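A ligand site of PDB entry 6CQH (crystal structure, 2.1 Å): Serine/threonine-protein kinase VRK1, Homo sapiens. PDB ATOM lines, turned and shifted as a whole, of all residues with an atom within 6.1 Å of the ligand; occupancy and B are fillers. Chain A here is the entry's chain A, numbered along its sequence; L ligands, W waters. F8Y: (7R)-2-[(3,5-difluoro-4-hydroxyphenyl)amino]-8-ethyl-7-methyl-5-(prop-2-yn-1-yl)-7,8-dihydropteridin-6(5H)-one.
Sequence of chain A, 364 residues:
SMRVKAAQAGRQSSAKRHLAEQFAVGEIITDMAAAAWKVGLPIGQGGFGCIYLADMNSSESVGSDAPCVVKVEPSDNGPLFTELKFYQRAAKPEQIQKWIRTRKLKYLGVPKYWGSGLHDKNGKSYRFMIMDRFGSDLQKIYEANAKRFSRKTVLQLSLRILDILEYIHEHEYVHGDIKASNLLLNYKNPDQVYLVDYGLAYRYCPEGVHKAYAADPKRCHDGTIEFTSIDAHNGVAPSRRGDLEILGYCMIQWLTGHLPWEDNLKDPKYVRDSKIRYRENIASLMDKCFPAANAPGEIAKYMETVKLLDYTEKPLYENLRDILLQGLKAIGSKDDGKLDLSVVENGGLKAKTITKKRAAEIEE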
ATOM      1  N   ILE A  43      28.258 -23.971  19.372  1.00  0.00           N
ATOM      2  CA  ILE A  43      28.744 -24.801  20.461  1.00  0.00           C
ATOM      3  C   ILE A  43      27.903 -26.067  20.657  1.00  0.00           C
ATOM      4  O   ILE A  43      26.696 -26.058  20.469  1.00  0.00           O
ATOM      5  CB  ILE A  43      28.738 -24.016  21.775  1.00  0.00           C
ATOM      6  CG1 ILE A  43      27.323 -23.516  22.063  1.00  0.00           C
ATOM      7  CG2 ILE A  43      29.700 -22.852  21.731  1.00  0.00           C
ATOM      8  CD1 ILE A  43      26.451 -24.555  22.711  1.00  0.00           C
ATOM      9  N   GLY A  44      28.576 -27.185  20.926  1.00  0.00           N
ATOM     10  CA  GLY A  44      27.916 -28.418  21.265  1.00  0.00           C
ATOM     11  C   GLY A  44      26.830 -28.991  20.310  1.00  0.00           C
ATOM     12  O   GLY A  44      25.864 -29.562  20.780  1.00  0.00           O
ATOM     13  N   PHE A  48      21.772 -27.062  22.200  1.00  0.00           N
ATOM     14  CA  PHE A  48      21.854 -25.801  22.957  1.00  0.00           C
ATOM     15  C   PHE A  48      21.517 -24.516  22.163  1.00  0.00           C
ATOM     16  O   PHE A  48      21.983 -23.436  22.526  1.00  0.00           O
ATOM     17  CB  PHE A  48      23.253 -25.664  23.589  1.00  0.00           C
ATOM     18  N   ILE A  51      23.650 -20.319  19.679  1.00  0.00           N
ATOM     19  CA  ILE A  51      24.767 -19.793  20.433  1.00  0.00           C
ATOM     20  C   ILE A  51      26.013 -20.231  19.688  1.00  0.00           C
ATOM     21  O   ILE A  51      26.164 -21.399  19.393  1.00  0.00           O
ATOM     22  CB  ILE A  51      24.802 -20.321  21.883  1.00  0.00           C
ATOM     23  CG1 ILE A  51      23.480 -19.990  22.604  1.00  0.00           C
ATOM     24  CG2 ILE A  51      25.996 -19.760  22.638  1.00  0.00           C
ATOM     25  CD1 ILE A  51      23.361 -20.531  24.019  1.00  0.00           C
ATOM     26  N   LEU A  53      30.493 -19.755  19.189  1.00  0.00           N
ATOM     27  CA  LEU A  53      31.768 -19.287  19.725  1.00  0.00           C
ATOM     28  C   LEU A  53      32.018 -17.874  19.194  1.00  0.00           C
ATOM     29  O   LEU A  53      31.551 -17.519  18.096  1.00  0.00           O
ATOM     30  CB  LEU A  53      32.932 -20.192  19.326  1.00  0.00           C
ATOM     31  CG  LEU A  53      32.905 -21.609  19.914  1.00  0.00           C
ATOM     32  CD1 LEU A  53      33.808 -22.531  19.110  1.00  0.00           C
ATOM     33  CD2 LEU A  53      33.313 -21.603  21.388  1.00  0.00           C
ATOM     34  N   SER A  64      38.280 -23.105  18.705  1.00  0.00           N
ATOM     35  CA  SER A  64      37.442 -23.931  19.587  1.00  0.00           C
ATOM     36  C   SER A  64      37.705 -23.688  21.083  1.00  0.00           C
ATOM     37  O   SER A  64      36.917 -24.096  21.925  1.00  0.00           O
ATOM     38  CB  SER A  64      37.579 -25.425  19.256  1.00  0.00           C
ATOM     39  OG  SER A  64      38.780 -25.965  19.778  1.00  0.00           O
ATOM     40  N   VAL A  69      30.970 -16.374  23.917  1.00  0.00           N
ATOM     41  CA  VAL A  69      29.940 -16.843  23.022  1.00  0.00           C
ATOM     42  C   VAL A  69      29.068 -15.667  22.649  1.00  0.00           C
ATOM     43  O   VAL A  69      28.958 -14.680  23.386  1.00  0.00           O
ATOM     44  CB  VAL A  69      29.058 -17.973  23.621  1.00  0.00           C
ATOM     45  CG1 VAL A  69      29.913 -19.168  24.014  1.00  0.00           C
ATOM     46  CG2 VAL A  69      28.221 -17.502  24.795  1.00  0.00           C
ATOM     47  N   LYS A  71      25.080 -15.099  21.705  1.00  0.00           N
ATOM     48  CA  LYS A  71      23.711 -15.577  21.682  1.00  0.00           C
ATOM     49  C   LYS A  71      22.955 -14.670  20.737  1.00  0.00           C
ATOM     50  O   LYS A  71      23.139 -13.448  20.783  1.00  0.00           O
ATOM     51  CB  LYS A  71      23.072 -15.476  23.048  1.00  0.00           C
ATOM     52  CG  LYS A  71      23.805 -16.283  24.105  1.00  0.00           C
ATOM     53  CD  LYS A  71      23.076 -16.274  25.442  1.00  0.00           C
ATOM     54  CE  LYS A  71      21.694 -16.907  25.344  1.00  0.00           C
ATOM     55  NZ  LYS A  71      21.200 -17.366  26.661  1.00  0.00           N
ATOM     56  N   GLU A  83      16.694 -11.356  29.460  1.00  0.00           N
ATOM     57  CA  GLU A  83      18.029 -11.769  29.861  1.00  0.00           C
ATOM     58  C   GLU A  83      19.053 -10.646  29.676  1.00  0.00           C
ATOM     59  O   GLU A  83      19.879 -10.406  30.556  1.00  0.00           O
ATOM     60  CB  GLU A  83      18.437 -13.019  29.066  1.00  0.00           C
ATOM     61  CG  GLU A  83      19.853 -13.490  29.310  1.00  0.00           C
ATOM     62  CD  GLU A  83      20.042 -14.919  28.860  1.00  0.00           C
ATOM     63  OE1 GLU A  83      20.005 -15.128  27.634  1.00  0.00           O
ATOM     64  OE2 GLU A  83      20.164 -15.834  29.725  1.00  0.00           O
ATOM     65  N   TYR A  87      21.403  -8.814  32.513  1.00  0.00           N
ATOM     66  CA  TYR A  87      22.860  -8.673  32.386  1.00  0.00           C
ATOM     67  C   TYR A  87      23.332  -7.198  32.441  1.00  0.00           C
ATOM     68  O   TYR A  87      24.256  -6.876  33.190  1.00  0.00           O
ATOM     69  CB  TYR A  87      23.375  -9.429  31.155  1.00  0.00           C
ATOM     70  CG  TYR A  87      23.488 -10.915  31.423  1.00  0.00           C
ATOM     71  CD1 TYR A  87      24.356 -11.390  32.415  1.00  0.00           C
ATOM     72  CD2 TYR A  87      22.747 -11.846  30.706  1.00  0.00           C
ATOM     73  CE1 TYR A  87      24.451 -12.740  32.703  1.00  0.00           C
ATOM     74  CE2 TYR A  87      22.859 -13.213  30.978  1.00  0.00           C
ATOM     75  CZ  TYR A  87      23.706 -13.646  31.987  1.00  0.00           C
ATOM     76  OH  TYR A  87      23.883 -14.973  32.269  1.00  0.00           O
ATOM     77  N   PRO A 111      27.552 -14.910  35.306  1.00  0.00           N
ATOM     78  CA  PRO A 111      28.332 -14.752  34.069  1.00  0.00           C
ATOM     79  C   PRO A 111      28.534 -13.298  33.688  1.00  0.00           C
ATOM     80  O   PRO A 111      27.646 -12.483  33.894  1.00  0.00           O
ATOM     81  CB  PRO A 111      27.469 -15.439  33.010  1.00  0.00           C
ATOM     82  CG  PRO A 111      26.641 -16.403  33.775  1.00  0.00           C
ATOM     83  CD  PRO A 111      26.377 -15.786  35.107  1.00  0.00           C
ATOM     84  N   LYS A 112      29.699 -12.983  33.134  1.00  0.00           N
ATOM     85  CA  LYS A 112      29.957 -11.614  32.686  1.00  0.00           C
ATOM     86  C   LYS A 112      29.343 -11.333  31.328  1.00  0.00           C
ATOM     87  O   LYS A 112      29.353 -12.174  30.440  1.00  0.00           O
ATOM     88  CB  LYS A 112      31.436 -11.284  32.717  1.00  0.00           C
ATOM     89  CG  LYS A 112      31.976 -11.461  34.126  1.00  0.00           C
ATOM     90  CD  LYS A 112      33.277 -10.733  34.409  1.00  0.00           C
ATOM     91  CE  LYS A 112      33.636 -11.008  35.864  1.00  0.00           C
ATOM     92  NZ  LYS A 112      34.966 -10.452  36.195  1.00  0.00           N
ATOM     93  N   MET A 131      28.755 -13.033  25.760  1.00  0.00           N
ATOM     94  CA  MET A 131      28.945 -13.522  27.125  1.00  0.00           C
ATOM     95  C   MET A 131      30.225 -14.315  27.277  1.00  0.00           C
ATOM     96  O   MET A 131      30.800 -14.748  26.307  1.00  0.00           O
ATOM     97  CB  MET A 131      27.810 -14.481  27.501  1.00  0.00           C
ATOM     98  CG  MET A 131      26.404 -13.916  27.315  1.00  0.00           C
ATOM     99  SD  MET A 131      26.145 -12.456  28.346  1.00  0.00           S
ATOM    100  CE  MET A 131      26.210 -13.197  29.980  1.00  0.00           C
ATOM    101  N   ASP A 132      30.630 -14.548  28.525  1.00  0.00           N
ATOM    102  CA  ASP A 132      31.641 -15.541  28.852  1.00  0.00           C
ATOM    103  C   ASP A 132      31.320 -16.914  28.229  1.00  0.00           C
ATOM    104  O   ASP A 132      30.155 -17.339  28.209  1.00  0.00           O
ATOM    105  CB  ASP A 132      31.729 -15.768  30.366  1.00  0.00           C
ATOM    106  CG  ASP A 132      32.487 -14.664  31.128  1.00  0.00           C
ATOM    107  OD1 ASP A 132      33.454 -14.078  30.586  1.00  0.00           O
ATOM    108  OD2 ASP A 132      32.111 -14.430  32.326  1.00  0.00           O
ATOM    109  N   ARG A 133      32.356 -17.593  27.746  1.00  0.00           N
ATOM    110  CA  ARG A 133      32.272 -18.992  27.352  1.00  0.00           C
ATOM    111  C   ARG A 133      32.627 -19.883  28.555  1.00  0.00           C
ATOM    112  O   ARG A 133      33.644 -19.669  29.200  1.00  0.00           O
ATOM    113  CB  ARG A 133      33.222 -19.269  26.184  1.00  0.00           C
ATOM    114  CG  ARG A 133      33.237 -20.705  25.688  1.00  0.00           C
ATOM    115  CD  ARG A 133      34.336 -21.514  26.343  1.00  0.00           C
ATOM    116  NE  ARG A 133      34.340 -22.891  25.888  1.00  0.00           N
ATOM    117  CZ  ARG A 133      34.916 -23.347  24.776  1.00  0.00           C
ATOM    118  NH1 ARG A 133      35.595 -22.534  23.947  1.00  0.00           N
ATOM    119  NH2 ARG A 133      34.828 -24.652  24.506  1.00  0.00           N
ATOM    120  N   PHE A 134      31.823 -20.904  28.808  1.00  0.00           N
ATOM    121  CA  PHE A 134      32.057 -21.859  29.908  1.00  0.00           C
ATOM    122  C   PHE A 134      32.461 -23.244  29.409  1.00  0.00           C
ATOM    123  O   PHE A 134      32.446 -23.502  28.223  1.00  0.00           O
ATOM    124  CB  PHE A 134      30.811 -21.932  30.771  1.00  0.00           C
ATOM    125  CG  PHE A 134      30.496 -20.629  31.437  1.00  0.00           C
ATOM    126  CD1 PHE A 134      31.306 -20.163  32.474  1.00  0.00           C
ATOM    127  CD2 PHE A 134      29.434 -19.841  31.017  1.00  0.00           C
ATOM    128  CE1 PHE A 134      31.061 -18.948  33.073  1.00  0.00           C
ATOM    129  CE2 PHE A 134      29.167 -18.629  31.619  1.00  0.00           C
ATOM    130  CZ  PHE A 134      29.990 -18.168  32.646  1.00  0.00           C
ATOM    131  N   GLY A 135      32.849 -24.121  30.320  1.00  0.00           N
ATOM    132  CA  GLY A 135      32.971 -25.539  30.014  1.00  0.00           C
ATOM    133  C   GLY A 135      31.642 -26.270  30.193  1.00  0.00           C
ATOM    134  O   GLY A 135      30.579 -25.780  29.822  1.00  0.00           O
ATOM    135  N   SER A 136      31.709 -27.438  30.798  1.00  0.00           N
ATOM    136  CA  SER A 136      30.567 -28.355  30.820  1.00  0.00           C
ATOM    137  C   SER A 136      29.492 -27.905  31.817  1.00  0.00           C
ATOM    138  O   SER A 136      29.779 -27.268  32.851  1.00  0.00           O
ATOM    139  CB  SER A 136      31.058 -29.777  31.146  1.00  0.00           C
ATOM    140  OG  SER A 136      30.002 -30.702  31.218  1.00  0.00           O
ATOM    141  N   ASP A 137      28.234 -28.219  31.498  1.00  0.00           N
ATOM    142  CA  ASP A 137      27.136 -28.068  32.481  1.00  0.00           C
ATOM    143  C   ASP A 137      27.201 -29.170  33.539  1.00  0.00           C
ATOM    144  O   ASP A 137      27.791 -30.213  33.304  1.00  0.00           O
ATOM    145  CB  ASP A 137      25.752 -27.992  31.791  1.00  0.00           C
ATOM    146  CG  ASP A 137      25.329 -29.287  31.166  1.00  0.00           C
ATOM    147  OD1 ASP A 137      24.889 -30.203  31.886  1.00  0.00           O
ATOM    148  OD2 ASP A 137      25.419 -29.386  29.937  1.00  0.00           O
ATOM    149  N   SER A 181      21.570 -28.453  34.816  1.00  0.00           N
ATOM    150  CA  SER A 181      21.786 -28.012  33.423  1.00  0.00           C
ATOM    151  C   SER A 181      21.962 -26.486  33.232  1.00  0.00           C
ATOM    152  O   SER A 181      22.459 -26.078  32.210  1.00  0.00           O
ATOM    153  CB  SER A 181      20.681 -28.534  32.470  1.00  0.00           C
ATOM    154  OG  SER A 181      19.432 -27.942  32.726  1.00  0.00           O
ATOM    155  N   LEU A 184      27.116 -24.055  35.018  1.00  0.00           N
ATOM    156  CA  LEU A 184      28.228 -24.298  34.115  1.00  0.00           C
ATOM    157  C   LEU A 184      29.532 -24.056  34.842  1.00  0.00           C
ATOM    158  O   LEU A 184      29.602 -23.205  35.729  1.00  0.00           O
ATOM    159  CB  LEU A 184      28.144 -23.373  32.894  1.00  0.00           C
ATOM    160  CG  LEU A 184      26.829 -23.347  32.132  1.00  0.00           C
ATOM    161  CD1 LEU A 184      26.930 -22.469  30.892  1.00  0.00           C
ATOM    162  CD2 LEU A 184      26.414 -24.744  31.724  1.00  0.00           C
ATOM    163  N   VAL A 196      23.519 -19.823  34.857  1.00  0.00           N
ATOM    164  CA  VAL A 196      23.099 -19.176  33.588  1.00  0.00           C
ATOM    165  C   VAL A 196      21.587 -19.265  33.382  1.00  0.00           C
ATOM    166  O   VAL A 196      20.867 -19.861  34.211  1.00  0.00           O
ATOM    167  CB  VAL A 196      23.850 -19.771  32.366  1.00  0.00           C
ATOM    168  CG1 VAL A 196      25.339 -19.865  32.662  1.00  0.00           C
ATOM    169  CG2 VAL A 196      23.311 -21.142  31.969  1.00  0.00           C
ATOM    170  N   ASP A 197      21.127 -18.657  32.275  1.00  0.00           N
ATOM    171  CA  ASP A 197      19.734 -18.576  31.845  1.00  0.00           C
ATOM    172  C   ASP A 197      18.908 -17.635  32.721  1.00  0.00           C
ATOM    173  O   ASP A 197      18.361 -18.037  33.757  1.00  0.00           O
ATOM    174  CB  ASP A 197      19.074 -19.968  31.729  1.00  0.00           C
ATOM    175  CG  ASP A 197      17.731 -19.938  30.967  1.00  0.00           C
ATOM    176  OD1 ASP A 197      17.112 -18.850  30.794  1.00  0.00           O
ATOM    177  OD2 ASP A 197      17.291 -21.020  30.538  1.00  0.00           O
ATOM    178  N   TYR A 198      18.830 -16.381  32.276  1.00  0.00           N
ATOM    179  CA  TYR A 198      17.967 -15.382  32.914  1.00  0.00           C
ATOM    180  C   TYR A 198      16.821 -14.939  31.993  1.00  0.00           C
ATOM    181  O   TYR A 198      16.217 -13.897  32.219  1.00  0.00           O
ATOM    182  CB  TYR A 198      18.827 -14.196  33.381  1.00  0.00           C
ATOM    183  CG  TYR A 198      19.844 -14.647  34.415  1.00  0.00           C
ATOM    184  CD1 TYR A 198      21.035 -15.228  34.018  1.00  0.00           C
ATOM    185  CD2 TYR A 198      19.588 -14.524  35.781  1.00  0.00           C
ATOM    186  CE1 TYR A 198      21.956 -15.683  34.954  1.00  0.00           C
ATOM    187  CE2 TYR A 198      20.510 -14.975  36.725  1.00  0.00           C
ATOM    188  CZ  TYR A 198      21.693 -15.560  36.298  1.00  0.00           C
ATOM    189  OH  TYR A 198      22.624 -16.000  37.215  1.00  0.00           O
HETATM  190  C4  F8Y L   1      25.765 -17.551  29.220  1.00  0.00           C
HETATM  191  C14 F8Y L   1      25.028 -23.823  26.746  1.00  0.00           C
HETATM  192  C5  F8Y L   1      26.906 -18.165  28.765  1.00  0.00           C
HETATM  193  C6  F8Y L   1      26.791 -19.189  27.824  1.00  0.00           C
HETATM  194  C11 F8Y L   1      26.698 -25.713  26.912  1.00  0.00           C
HETATM  195  C7  F8Y L   1      28.218 -21.156  27.184  1.00  0.00           C
HETATM  196  C8  F8Y L   1      27.478 -23.331  26.926  1.00  0.00           C
HETATM  197  C9  F8Y L   1      28.827 -23.776  26.795  1.00  0.00           C
HETATM  198  C10 F8Y L   1      29.806 -22.770  26.859  1.00  0.00           C
HETATM  199  C12 F8Y L   1      28.116 -26.106  26.513  1.00  0.00           C
HETATM  200  C13 F8Y L   1      26.350 -26.293  28.277  1.00  0.00           C
HETATM  201  N1  F8Y L   1      27.964 -19.828  27.377  1.00  0.00           N
HETATM  202  N2  F8Y L   1      27.191 -22.027  27.122  1.00  0.00           N
HETATM  203  C3  F8Y L   1      24.494 -17.919  28.772  1.00  0.00           C
HETATM  204  N3  F8Y L   1      29.515 -21.492  27.066  1.00  0.00           N
HETATM  205  C1  F8Y L   1      25.531 -19.579  27.363  1.00  0.00           C
HETATM  206  C2  F8Y L   1      24.417 -18.935  27.846  1.00  0.00           C
HETATM  207  F1  F8Y L   1      25.876 -16.547  30.116  1.00  0.00           F
HETATM  208  O1  F8Y L   1      23.372 -17.319  29.220  1.00  0.00           O
HETATM  209  F2  F8Y L   1      23.194 -19.317  27.399  1.00  0.00           F
HETATM  210  N4  F8Y L   1      26.426 -24.259  26.868  1.00  0.00           N
HETATM  211  N5  F8Y L   1      29.108 -25.153  26.588  1.00  0.00           N
HETATM  212  O2  F8Y L   1      28.342 -27.246  26.134  1.00  0.00           O
HETATM  213  C15 F8Y L   1      24.346 -23.544  28.074  1.00  0.00           C
HETATM  214  C16 F8Y L   1      30.499 -25.599  26.398  1.00  0.00           C
HETATM  215  C17 F8Y L   1      31.036 -25.266  25.077  1.00  0.00           C
HETATM  216  C18 F8Y L   1      31.452 -24.949  24.012  1.00  0.00           C
HETATM  217  O   HOH W   1      21.652 -23.795  29.982  1.00  0.00           O
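The side-chain amino group (NZ) of Lys 71 sits at hydrogen-bond distance from an oxygen (O1) of the ligand.
O of Asp 132 lies close to N1 of the ligand, at 3.4 Å.
N3 of the ligand is in hydrogen-bond range of N of Phe 134.
The backbone NH of Tyr 198 sits at hydrogen-bond distance from the side-chain carboxylate of Glu 83 (2.9 Å).
The side-chain amino group of Lys 71 lies within salt-bridge range of the side-chain carboxylate of Glu 83 (2.7 Å).
The backbone carbonyl oxygen of Ile 51 sits at hydrogen-bond distance from the backbone NH of Ile 43, at 3.3 Å.
NH1 of Arg 133 sits at hydrogen-bond distance from O of Ser 64 (2.9 Å).
The backbone NH of Lys 112 lies within hydrogen-bond range of the side-chain carboxylate of Asp 132, 2.9 Å away.
The backbone NH (N) of Val 69 lies within hydrogen-bond range of the backbone carbonyl oxygen (O) of Met 131, 2.9 Å away.
OH of Tyr 87 lies close to F1 of the ligand (3.3 Å).
CG2 of Ile 43 touches C18 of the ligand (3.6 Å).
Ile 51 touches the ligand.
Val 69 touches the ligand.
Glu 83 touches the ligand.
CB of Pro 111 touches F1 of the ligand (3.5 Å).
CE of Met 131 touches F1 of the ligand, at 3.4 Å.
NH2 of Arg 133 touches C18 of the ligand, 3.4 Å away.
Gly 135 touches the ligand (O to C16, 3.4 Å).
Asp 137 touches the ligand (OD2 to C13, 3.6 Å).
Leu 184 touches the ligand (CD2 to C13, 3.8 Å).
Hydrophobic or aromatic side chains that line the ligand: Ile 43, Ile 51, Val 69, Pro 111, Met 131, Phe 134 and Leu 184.
Within 4 Å of the ligand: Ile 43, Ile 51, Val 69, Lys 71, Glu 83, Tyr 87, Pro 111, Met 131, Asp 132, Arg 133, Phe 134, Gly 135, Asp 137 and Leu 184.
The nearest printed residue that does not touch the ligand is Val 196 (4.02 Å).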
